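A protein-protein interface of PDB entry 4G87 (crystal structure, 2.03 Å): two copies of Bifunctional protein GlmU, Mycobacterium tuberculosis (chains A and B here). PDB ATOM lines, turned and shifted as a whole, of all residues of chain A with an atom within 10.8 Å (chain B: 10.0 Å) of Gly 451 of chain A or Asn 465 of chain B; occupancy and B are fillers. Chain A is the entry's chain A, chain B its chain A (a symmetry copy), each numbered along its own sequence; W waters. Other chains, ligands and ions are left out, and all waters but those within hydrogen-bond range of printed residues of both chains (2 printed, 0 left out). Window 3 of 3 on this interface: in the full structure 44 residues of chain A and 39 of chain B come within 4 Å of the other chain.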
ATOM      1  N   SER A 393     -20.991  21.081 -28.987  1.00  0.00           N
ATOM      2  CA  SER A 393     -20.274  21.667 -27.854  1.00  0.00           C
ATOM      3  C   SER A 393     -21.205  21.777 -26.640  1.00  0.00           C
ATOM      4  O   SER A 393     -22.457  21.636 -26.766  1.00  0.00           O
ATOM      5  CB  SER A 393     -19.742  23.011 -28.270  1.00  0.00           C
ATOM      6  OG  SER A 393     -18.642  22.862 -29.155  1.00  0.00           O
ATOM      7  N   VAL A 414     -16.218  29.930 -30.478  1.00  0.00           N
ATOM      8  CA  VAL A 414     -15.953  28.731 -29.739  1.00  0.00           C
ATOM      9  C   VAL A 414     -16.116  27.610 -30.725  1.00  0.00           C
ATOM     10  O   VAL A 414     -17.147  27.546 -31.393  1.00  0.00           O
ATOM     11  CB  VAL A 414     -17.022  28.546 -28.570  1.00  0.00           C
ATOM     12  CG1 VAL A 414     -16.859  27.174 -27.915  1.00  0.00           C
ATOM     13  CG2 VAL A 414     -16.849  29.682 -27.505  1.00  0.00           C
ATOM     14  N   GLY A 415     -15.160  26.671 -30.776  1.00  0.00           N
ATOM     15  CA  GLY A 415     -15.199  25.582 -31.800  1.00  0.00           C
ATOM     16  C   GLY A 415     -16.158  24.453 -31.474  1.00  0.00           C
ATOM     17  O   GLY A 415     -17.053  24.611 -30.672  1.00  0.00           O
ATOM     18  N   SER A 416     -15.986  23.313 -32.124  1.00  0.00           N
ATOM     19  CA  SER A 416     -16.826  22.166 -31.984  1.00  0.00           C
ATOM     20  C   SER A 416     -16.281  21.212 -30.928  1.00  0.00           C
ATOM     21  O   SER A 416     -15.085  21.237 -30.660  1.00  0.00           O
ATOM     22  CB  SER A 416     -16.905  21.442 -33.324  1.00  0.00           C
ATOM     23  OG  SER A 416     -17.480  22.326 -34.256  1.00  0.00           O
ATOM     24  N   HIS A 417     -17.162  20.405 -30.345  1.00  0.00           N
ATOM     25  CA  HIS A 417     -16.866  19.400 -29.296  1.00  0.00           C
ATOM     26  C   HIS A 417     -16.176  20.039 -28.091  1.00  0.00           C
ATOM     27  O   HIS A 417     -15.511  19.344 -27.343  1.00  0.00           O
ATOM     28  CB  HIS A 417     -16.021  18.223 -29.854  1.00  0.00           C
ATOM     29  CG  HIS A 417     -16.655  17.560 -31.038  1.00  0.00           C
ATOM     30  ND1 HIS A 417     -17.538  16.505 -30.910  1.00  0.00           N
ATOM     31  CD2 HIS A 417     -16.592  17.850 -32.360  1.00  0.00           C
ATOM     32  CE1 HIS A 417     -17.961  16.154 -32.110  1.00  0.00           C
ATOM     33  NE2 HIS A 417     -17.397  16.953 -33.002  1.00  0.00           N
ATOM     34  N   VAL A 418     -16.323  21.348 -27.927  1.00  0.00           N
ATOM     35  CA  VAL A 418     -15.835  22.037 -26.725  1.00  0.00           C
ATOM     36  C   VAL A 418     -16.698  21.695 -25.457  1.00  0.00           C
ATOM     37  O   VAL A 418     -17.926  21.529 -25.575  1.00  0.00           O
ATOM     38  CB  VAL A 418     -15.845  23.508 -27.012  1.00  0.00           C
ATOM     39  CG1 VAL A 418     -15.544  24.330 -25.796  1.00  0.00           C
ATOM     40  CG2 VAL A 418     -14.871  23.796 -28.125  1.00  0.00           C
ATOM     41  N   ARG A 419     -16.077  21.569 -24.264  1.00  0.00           N
ATOM     42  CA  ARG A 419     -16.863  21.479 -23.035  1.00  0.00           C
ATOM     43  C   ARG A 419     -16.345  22.512 -22.065  1.00  0.00           C
ATOM     44  O   ARG A 419     -15.215  22.365 -21.549  1.00  0.00           O
ATOM     45  CB  ARG A 419     -16.742  20.113 -22.384  1.00  0.00           C
ATOM     46  CG  ARG A 419     -17.052  18.969 -23.341  1.00  0.00           C
ATOM     47  CD  ARG A 419     -17.395  17.751 -22.589  1.00  0.00           C
ATOM     48  NE  ARG A 419     -18.728  17.274 -22.952  1.00  0.00           N
ATOM     49  CZ  ARG A 419     -19.751  17.203 -22.094  1.00  0.00           C
ATOM     50  NH1 ARG A 419     -19.604  17.597 -20.820  1.00  0.00           N
ATOM     51  NH2 ARG A 419     -20.927  16.722 -22.505  1.00  0.00           N
ATOM     52  N   THR A 431     -10.934  33.213 -28.823  1.00  0.00           N
ATOM     53  CA  THR A 431     -11.224  32.028 -29.625  1.00  0.00           C
ATOM     54  C   THR A 431     -10.956  30.763 -28.849  1.00  0.00           C
ATOM     55  O   THR A 431      -9.856  30.613 -28.244  1.00  0.00           O
ATOM     56  CB  THR A 431     -10.384  32.053 -30.883  1.00  0.00           C
ATOM     57  OG1 THR A 431     -10.689  33.273 -31.575  1.00  0.00           O
ATOM     58  CG2 THR A 431     -10.696  30.845 -31.753  1.00  0.00           C
ATOM     59  N   ILE A 432     -11.925  29.846 -28.824  1.00  0.00           N
ATOM     60  CA  ILE A 432     -11.708  28.587 -28.088  1.00  0.00           C
ATOM     61  C   ILE A 432     -11.692  27.513 -29.131  1.00  0.00           C
ATOM     62  O   ILE A 432     -12.685  27.325 -29.823  1.00  0.00           O
ATOM     63  CB  ILE A 432     -12.823  28.264 -27.044  1.00  0.00           C
ATOM     64  CG1 ILE A 432     -13.139  29.455 -26.130  1.00  0.00           C
ATOM     65  CG2 ILE A 432     -12.521  26.939 -26.268  1.00  0.00           C
ATOM     66  CD1 ILE A 432     -12.062  29.945 -25.373  1.00  0.00           C
ATOM     67  N   GLY A 433     -10.549  26.829 -29.256  1.00  0.00           N
ATOM     68  CA  GLY A 433     -10.391  25.789 -30.250  1.00  0.00           C
ATOM     69  C   GLY A 433     -11.186  24.547 -30.023  1.00  0.00           C
ATOM     70  O   GLY A 433     -11.621  24.230 -28.875  1.00  0.00           O
ATOM     71  N   ASP A 434     -11.346  23.782 -31.111  1.00  0.00           N
ATOM     72  CA  ASP A 434     -12.093  22.571 -31.088  1.00  0.00           C
ATOM     73  C   ASP A 434     -11.630  21.636 -29.985  1.00  0.00           C
ATOM     74  O   ASP A 434     -10.416  21.443 -29.803  1.00  0.00           O
ATOM     75  CB  ASP A 434     -11.928  21.810 -32.425  1.00  0.00           C
ATOM     76  CG  ASP A 434     -12.638  22.503 -33.615  1.00  0.00           C
ATOM     77  OD1 ASP A 434     -13.483  23.445 -33.449  1.00  0.00           O
ATOM     78  OD2 ASP A 434     -12.346  22.065 -34.745  1.00  0.00           O
ATOM     79  N   GLY A 435     -12.576  20.981 -29.307  1.00  0.00           N
ATOM     80  CA  GLY A 435     -12.254  19.959 -28.319  1.00  0.00           C
ATOM     81  C   GLY A 435     -11.629  20.522 -27.031  1.00  0.00           C
ATOM     82  O   GLY A 435     -11.315  19.722 -26.135  1.00  0.00           O
ATOM     83  N   ALA A 436     -11.421  21.857 -26.931  1.00  0.00           N
ATOM     84  CA  ALA A 436     -10.972  22.504 -25.645  1.00  0.00           C
ATOM     85  C   ALA A 436     -11.995  22.392 -24.499  1.00  0.00           C
ATOM     86  O   ALA A 436     -13.210  22.233 -24.728  1.00  0.00           O
ATOM     87  CB  ALA A 436     -10.576  23.935 -25.829  1.00  0.00           C
ATOM     88  N   TYR A 437     -11.481  22.474 -23.272  1.00  0.00           N
ATOM     89  CA  TYR A 437     -12.262  22.431 -22.042  1.00  0.00           C
ATOM     90  C   TYR A 437     -11.892  23.698 -21.282  1.00  0.00           C
ATOM     91  O   TYR A 437     -10.798  24.251 -21.439  1.00  0.00           O
ATOM     92  CB  TYR A 437     -11.805  21.252 -21.153  1.00  0.00           C
ATOM     93  CG  TYR A 437     -12.544  19.931 -21.290  1.00  0.00           C
ATOM     94  CD1 TYR A 437     -13.102  19.320 -20.186  1.00  0.00           C
ATOM     95  CD2 TYR A 437     -12.667  19.289 -22.525  1.00  0.00           C
ATOM     96  CE1 TYR A 437     -13.804  18.066 -20.298  1.00  0.00           C
ATOM     97  CE2 TYR A 437     -13.344  18.066 -22.646  1.00  0.00           C
ATOM     98  CZ  TYR A 437     -13.895  17.458 -21.540  1.00  0.00           C
ATOM     99  OH  TYR A 437     -14.557  16.249 -21.669  1.00  0.00           O
ATOM    100  N   THR A 438     -12.768  24.105 -20.382  1.00  0.00           N
ATOM    101  CA  THR A 438     -12.489  25.201 -19.434  1.00  0.00           C
ATOM    102  C   THR A 438     -12.812  24.638 -18.063  1.00  0.00           C
ATOM    103  O   THR A 438     -13.738  23.884 -17.959  1.00  0.00           O
ATOM    104  CB  THR A 438     -13.501  26.264 -19.887  1.00  0.00           C
ATOM    105  OG1 THR A 438     -12.878  27.235 -20.729  1.00  0.00           O
ATOM    106  CG2 THR A 438     -14.389  26.737 -18.892  1.00  0.00           C
ATOM    107  N   ASP A 447      -7.059  33.421 -25.939  1.00  0.00           N
ATOM    108  CA  ASP A 447      -7.294  32.248 -26.760  1.00  0.00           C
ATOM    109  C   ASP A 447      -6.915  30.968 -26.073  1.00  0.00           C
ATOM    110  O   ASP A 447      -6.010  30.959 -25.234  1.00  0.00           O
ATOM    111  CB  ASP A 447      -6.552  32.399 -28.071  1.00  0.00           C
ATOM    112  CG  ASP A 447      -7.149  33.507 -28.943  1.00  0.00           C
ATOM    113  OD1 ASP A 447      -8.191  34.160 -28.569  1.00  0.00           O
ATOM    114  OD2 ASP A 447      -6.530  33.750 -30.001  1.00  0.00           O
ATOM    115  N   VAL A 448      -7.635  29.890 -26.390  1.00  0.00           N
ATOM    116  CA  VAL A 448      -7.442  28.593 -25.778  1.00  0.00           C
ATOM    117  C   VAL A 448      -7.243  27.684 -26.996  1.00  0.00           C
ATOM    118  O   VAL A 448      -8.169  27.503 -27.812  1.00  0.00           O
ATOM    119  CB  VAL A 448      -8.683  28.135 -24.958  1.00  0.00           C
ATOM    120  CG1 VAL A 448      -8.537  26.654 -24.461  1.00  0.00           C
ATOM    121  CG2 VAL A 448      -8.913  29.055 -23.768  1.00  0.00           C
ATOM    122  N   PRO A 449      -6.015  27.144 -27.168  1.00  0.00           N
ATOM    123  CA  PRO A 449      -5.762  26.144 -28.224  1.00  0.00           C
ATOM    124  C   PRO A 449      -6.716  24.946 -28.234  1.00  0.00           C
ATOM    125  O   PRO A 449      -7.235  24.524 -27.191  1.00  0.00           O
ATOM    126  CB  PRO A 449      -4.322  25.655 -27.947  1.00  0.00           C
ATOM    127  CG  PRO A 449      -3.645  26.839 -27.299  1.00  0.00           C
ATOM    128  CD  PRO A 449      -4.797  27.497 -26.428  1.00  0.00           C
ATOM    129  N   PRO A 450      -6.939  24.362 -29.426  1.00  0.00           N
ATOM    130  CA  PRO A 450      -7.710  23.116 -29.501  1.00  0.00           C
ATOM    131  C   PRO A 450      -7.186  22.048 -28.505  1.00  0.00           C
ATOM    132  O   PRO A 450      -5.939  21.874 -28.330  1.00  0.00           O
ATOM    133  CB  PRO A 450      -7.488  22.662 -30.975  1.00  0.00           C
ATOM    134  CG  PRO A 450      -7.225  23.886 -31.712  1.00  0.00           C
ATOM    135  CD  PRO A 450      -6.426  24.777 -30.755  1.00  0.00           C
ATOM    136  N   GLY A 451      -8.099  21.359 -27.831  1.00  0.00           N
ATOM    137  CA  GLY A 451      -7.707  20.290 -26.884  1.00  0.00           C
ATOM    138  C   GLY A 451      -6.968  20.762 -25.625  1.00  0.00           C
ATOM    139  O   GLY A 451      -6.538  19.923 -24.815  1.00  0.00           O
ATOM    140  N   ALA A 452      -6.792  22.072 -25.458  1.00  0.00           N
ATOM    141  CA  ALA A 452      -6.198  22.623 -24.254  1.00  0.00           C
ATOM    142  C   ALA A 452      -7.279  22.682 -23.125  1.00  0.00           C
ATOM    143  O   ALA A 452      -8.494  22.702 -23.400  1.00  0.00           O
ATOM    144  CB  ALA A 452      -5.665  24.041 -24.551  1.00  0.00           C
ATOM    145  N   LEU A 453      -6.858  22.674 -21.870  1.00  0.00           N
ATOM    146  CA  LEU A 453      -7.771  22.991 -20.788  1.00  0.00           C
ATOM    147  C   LEU A 453      -7.344  24.370 -20.239  1.00  0.00           C
ATOM    148  O   LEU A 453      -6.159  24.556 -19.950  1.00  0.00           O
ATOM    149  CB  LEU A 453      -7.798  21.888 -19.690  1.00  0.00           C
ATOM    150  CG  LEU A 453      -8.297  22.350 -18.313  1.00  0.00           C
ATOM    151  CD1 LEU A 453      -9.851  22.485 -18.221  1.00  0.00           C
ATOM    152  CD2 LEU A 453      -7.846  21.469 -17.155  1.00  0.00           C
ATOM    153  N   ALA A 454      -8.286  25.334 -20.149  1.00  0.00           N
ATOM    154  CA  ALA A 454      -8.015  26.680 -19.625  1.00  0.00           C
ATOM    155  C   ALA A 454      -8.600  26.778 -18.222  1.00  0.00           C
ATOM    156  O   ALA A 454      -9.753  26.349 -17.960  1.00  0.00           O
ATOM    157  CB  ALA A 454      -8.564  27.788 -20.545  1.00  0.00           C
ATOM    158  N   VAL A 455      -7.789  27.258 -17.288  1.00  0.00           N
ATOM    159  CA  VAL A 455      -8.230  27.336 -15.872  1.00  0.00           C
ATOM    160  C   VAL A 455      -7.808  28.674 -15.295  1.00  0.00           C
ATOM    161  O   VAL A 455      -6.930  29.337 -15.837  1.00  0.00           O
ATOM    162  CB  VAL A 455      -7.619  26.198 -14.978  1.00  0.00           C
ATOM    163  CG1 VAL A 455      -8.164  24.826 -15.382  1.00  0.00           C
ATOM    164  CG2 VAL A 455      -6.034  26.227 -14.998  1.00  0.00           C
ATOM    165  N   ASN B 462      -3.403  28.177 -19.639  1.00  0.00           N
ATOM    166  CA  ASN B 462      -3.792  27.096 -20.576  1.00  0.00           C
ATOM    167  C   ASN B 462      -2.936  25.859 -20.387  1.00  0.00           C
ATOM    168  O   ASN B 462      -1.721  25.977 -20.385  1.00  0.00           O
ATOM    169  CB  ASN B 462      -3.643  27.516 -22.037  1.00  0.00           C
ATOM    170  CG  ASN B 462      -4.675  28.587 -22.419  1.00  0.00           C
ATOM    171  OD1 ASN B 462      -5.703  28.713 -21.746  1.00  0.00           O
ATOM    172  ND2 ASN B 462      -4.394  29.359 -23.457  1.00  0.00           N
ATOM    173  N   ILE B 463      -3.567  24.690 -20.315  1.00  0.00           N
ATOM    174  CA  ILE B 463      -2.858  23.414 -20.143  1.00  0.00           C
ATOM    175  C   ILE B 463      -2.959  22.666 -21.466  1.00  0.00           C
ATOM    176  O   ILE B 463      -3.996  22.015 -21.746  1.00  0.00           O
ATOM    177  CB  ILE B 463      -3.480  22.590 -19.018  1.00  0.00           C
ATOM    178  CG1 ILE B 463      -3.440  23.374 -17.711  1.00  0.00           C
ATOM    179  CG2 ILE B 463      -2.778  21.233 -18.834  1.00  0.00           C
ATOM    180  CD1 ILE B 463      -4.307  22.775 -16.624  1.00  0.00           C
ATOM    181  N   GLU B 464      -1.904  22.758 -22.275  1.00  0.00           N
ATOM    182  CA  GLU B 464      -1.935  22.176 -23.609  1.00  0.00           C
ATOM    183  C   GLU B 464      -2.051  20.658 -23.619  1.00  0.00           C
ATOM    184  O   GLU B 464      -1.444  19.971 -22.777  1.00  0.00           O
ATOM    185  CB  GLU B 464      -0.739  22.654 -24.434  1.00  0.00           C
ATOM    186  CG  GLU B 464      -0.725  24.188 -24.573  1.00  0.00           C
ATOM    187  CD  GLU B 464      -0.279  24.687 -25.940  1.00  0.00           C
ATOM    188  OE1 GLU B 464      -0.625  24.069 -26.992  1.00  0.00           O
ATOM    189  OE2 GLU B 464       0.394  25.726 -25.974  1.00  0.00           O
ATOM    190  N   ASN B 465      -2.861  20.149 -24.558  1.00  0.00           N
ATOM    191  CA  ASN B 465      -3.086  18.710 -24.745  1.00  0.00           C
ATOM    192  C   ASN B 465      -3.676  18.015 -23.570  1.00  0.00           C
ATOM    193  O   ASN B 465      -3.548  16.771 -23.463  1.00  0.00           O
ATOM    194  CB  ASN B 465      -1.775  18.013 -25.161  1.00  0.00           C
ATOM    195  CG  ASN B 465      -1.183  18.618 -26.445  1.00  0.00           C
ATOM    196  OD1 ASN B 465      -1.722  18.427 -27.529  1.00  0.00           O
ATOM    197  ND2 ASN B 465      -0.081  19.376 -26.308  1.00  0.00           N
ATOM    198  N   TRP B 466      -4.324  18.767 -22.664  1.00  0.00           N
ATOM    199  CA  TRP B 466      -4.943  18.159 -21.476  1.00  0.00           C
ATOM    200  C   TRP B 466      -5.985  17.090 -21.860  1.00  0.00           C
ATOM    201  O   TRP B 466      -6.101  15.989 -21.213  1.00  0.00           O
ATOM    202  CB  TRP B 466      -5.554  19.227 -20.579  1.00  0.00           C
ATOM    203  CG  TRP B 466      -6.158  18.716 -19.351  1.00  0.00           C
ATOM    204  CD1 TRP B 466      -5.550  18.593 -18.118  1.00  0.00           C
ATOM    205  CD2 TRP B 466      -7.502  18.258 -19.191  1.00  0.00           C
ATOM    206  NE1 TRP B 466      -6.447  18.078 -17.200  1.00  0.00           N
ATOM    207  CE2 TRP B 466      -7.647  17.850 -17.835  1.00  0.00           C
ATOM    208  CE3 TRP B 466      -8.608  18.146 -20.062  1.00  0.00           C
ATOM    209  CZ2 TRP B 466      -8.861  17.356 -17.321  1.00  0.00           C
ATOM    210  CZ3 TRP B 466      -9.795  17.632 -19.556  1.00  0.00           C
ATOM    211  CH2 TRP B 466      -9.922  17.252 -18.197  1.00  0.00           C
ATOM    212  N   VAL B 467      -6.727  17.416 -22.915  1.00  0.00           N
ATOM    213  CA  VAL B 467      -7.808  16.586 -23.364  1.00  0.00           C
ATOM    214  C   VAL B 467      -7.303  15.257 -23.984  1.00  0.00           C
ATOM    215  O   VAL B 467      -7.901  14.215 -23.711  1.00  0.00           O
ATOM    216  CB  VAL B 467      -8.798  17.361 -24.351  1.00  0.00           C
ATOM    217  CG1 VAL B 467      -9.991  16.497 -24.718  1.00  0.00           C
ATOM    218  CG2 VAL B 467      -9.323  18.649 -23.711  1.00  0.00           C
ATOM    219  N   GLN B 468      -6.250  15.305 -24.817  1.00  0.00           N
ATOM    220  CA  GLN B 468      -5.614  14.088 -25.342  1.00  0.00           C
ATOM    221  C   GLN B 468      -5.288  13.195 -24.154  1.00  0.00           C
ATOM    222  O   GLN B 468      -5.582  11.997 -24.199  1.00  0.00           O
ATOM    223  CB  GLN B 468      -4.314  14.340 -26.114  1.00  0.00           C
ATOM    224  CG  GLN B 468      -4.379  15.262 -27.356  1.00  0.00           C
ATOM    225  CD  GLN B 468      -5.119  14.663 -28.584  1.00  0.00           C
ATOM    226  OE1 GLN B 468      -5.260  13.425 -28.728  1.00  0.00           O
ATOM    227  NE2 GLN B 468      -5.580  15.554 -29.483  1.00  0.00           N
ATOM    228  N   ARG B 469      -4.724  13.767 -23.078  1.00  0.00           N
ATOM    229  CA  ARG B 469      -4.276  12.945 -21.919  1.00  0.00           C
ATOM    230  C   ARG B 469      -5.381  12.417 -21.005  1.00  0.00           C
ATOM    231  O   ARG B 469      -5.303  11.268 -20.544  1.00  0.00           O
ATOM    232  CB  ARG B 469      -3.244  13.694 -21.051  1.00  0.00           C
ATOM    233  CG  ARG B 469      -2.011  14.089 -21.816  1.00  0.00           C
ATOM    234  CD  ARG B 469      -0.922  14.606 -20.894  1.00  0.00           C
ATOM    235  NE  ARG B 469      -1.230  15.890 -20.232  1.00  0.00           N
ATOM    236  CZ  ARG B 469      -0.856  17.080 -20.700  1.00  0.00           C
ATOM    237  NH1 ARG B 469      -0.184  17.163 -21.847  1.00  0.00           N
ATOM    238  NH2 ARG B 469      -1.141  18.194 -20.016  1.00  0.00           N
ATOM    239  N   LYS B 470      -6.367  13.271 -20.713  1.00  0.00           N
ATOM    240  CA  LYS B 470      -7.365  12.987 -19.675  1.00  0.00           C
ATOM    241  C   LYS B 470      -8.726  12.603 -20.228  1.00  0.00           C
ATOM    242  O   LYS B 470      -9.528  12.029 -19.493  1.00  0.00           O
ATOM    243  CB  LYS B 470      -7.499  14.154 -18.681  1.00  0.00           C
ATOM    244  CG  LYS B 470      -6.354  14.244 -17.701  1.00  0.00           C
ATOM    245  CD  LYS B 470      -6.477  13.159 -16.610  1.00  0.00           C
ATOM    246  CE  LYS B 470      -5.105  12.743 -16.099  1.00  0.00           C
ATOM    247  NZ  LYS B 470      -4.609  13.548 -14.903  1.00  0.00           N
HETATM  248  O   HOH W   1      -5.718  17.522 -26.103  1.00  0.00           O
HETATM  249  O   HOH W   2      -3.809  21.879 -26.624  1.00  0.00           O
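No position is printed for both chains.
Of the 9 printed residues of chain B, 5 touch a printed residue of chain A.
Gly 433 of chain A touches none of the printed residues of chain B. Gly 435 of chain A touches just one residue of chain B: Val 467 (3.3 Å). Ala 436 of chain A touches none of the printed residues of chain B. Printed residues of chain B within 4 Å of Val 448 of chain A: Asn 462 (3.8 Å). Of the printed residues of chain A, Asn 462 of chain B touches Asp 447, Val 448, Pro 449, Leu 453 and Ala 454. Asn 465 of chain B touches one residue of chain A. Printed residues of chain A within 4 Å of Trp 466 of chain B: Tyr 437, Gly 451 and Leu 453. Of chain A, only Gly 435, Tyr 437 and Gly 451 come within 4 Å of Val 467 of chain B. The nearest residue of chain A that does not touch Asn 465 of chain B is Ala 452 of chain A (4.2 Å). The nearest printed residue of chain A that does not touch Trp 466 of chain B is Ala 452 of chain A (4.6 Å).
Water W1 lies within hydrogen-bond range of N of Gln 468 of chain B (2.6 Å), O of Gly 451 of chain A (2.8 Å), N of Val 467 of chain B (3.3 Å) and O of Asn 465 of chain B (3.5 Å). Water W2 lies within hydrogen-bond range of the backbone carbonyl oxygen of Pro 450 of chain A (2.7 Å), the backbone NH of Asn 465 of chain B (2.9 Å) and the backbone NH of Ala 452 of chain A (3.2 Å).
Gly 435 of chain A touches Val 467 of chain B. CD1 of Tyr 437 of chain A touches CZ3 of Trp 466 of chain B, 3.8 Å away. Tyr 437 of chain A touches Val 467 of chain B. Val 448 of chain A touches Asn 462 of chain B (CG2 to OD1, 3.8 Å). Asn 462 of chain B touches Pro 449 of chain A (ND2 to CD, 3.5 Å). Asn 465 of chain B touches Gly 451 of chain A (C to O, 3.7 Å). O of Ile 463 of chain B touches CA of Ala 452 of chain A, 3.4 Å away. C of Asn 462 of chain B touches O of Leu 453 of chain A, 3.5 Å away. Leu 453 of chain A touches Trp 466 of chain B (CB to CG, 3.6 Å). Ala 454 of chain A touches Asn 462 of chain B.
The backbone carbonyl oxygen (O) of Thr 431 of chain A sits at hydrogen-bond distance from the backbone NH (N) of Val 448 of chain A, at 3.0 Å. The backbone carbonyl oxygen (O) of Asp 434 of chain A is in hydrogen-bond range of the backbone NH (N) of Gly 451 of chain A (3.0 Å). The backbone carbonyl oxygen (O) of Ser 416 of chain A sits at hydrogen-bond distance from the backbone NH (N) of Gly 435 of chain A (2.9 Å). The backbone NH (N) of Thr 431 of chain A is in hydrogen-bond range of the side-chain carboxylate (OD1) of Asp 447 of chain A (2.9 Å). N of Gly 433 of chain A lies within hydrogen-bond range of O of Val 448 of chain A, 2.9 Å away. The backbone NH (N) of Tyr 437 of chain A lies within hydrogen-bond range of the backbone carbonyl oxygen (O) of Ala 452 of chain A, at 3.0 Å.
The backbone NH (N) of Trp 466 of chain B sits at hydrogen-bond distance from the backbone carbonyl oxygen (O) of Gly 451 of chain A (3.3 Å). The backbone NH (N) of Ile 463 of chain B is in hydrogen-bond range of the backbone carbonyl oxygen (O) of Leu 453 of chain A, 2.6 Å away. The side-chain amide nitrogen (ND2) of Asn 462 of chain B is in hydrogen-bond range of the backbone carbonyl oxygen (O) of Asp 447 of chain A (2.9 Å). The backbone carbonyl oxygen (O) of Gly 451 of chain A sits at hydrogen-bond distance from the backbone NH (N) of Val 467 of chain B, 3.2 Å away.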
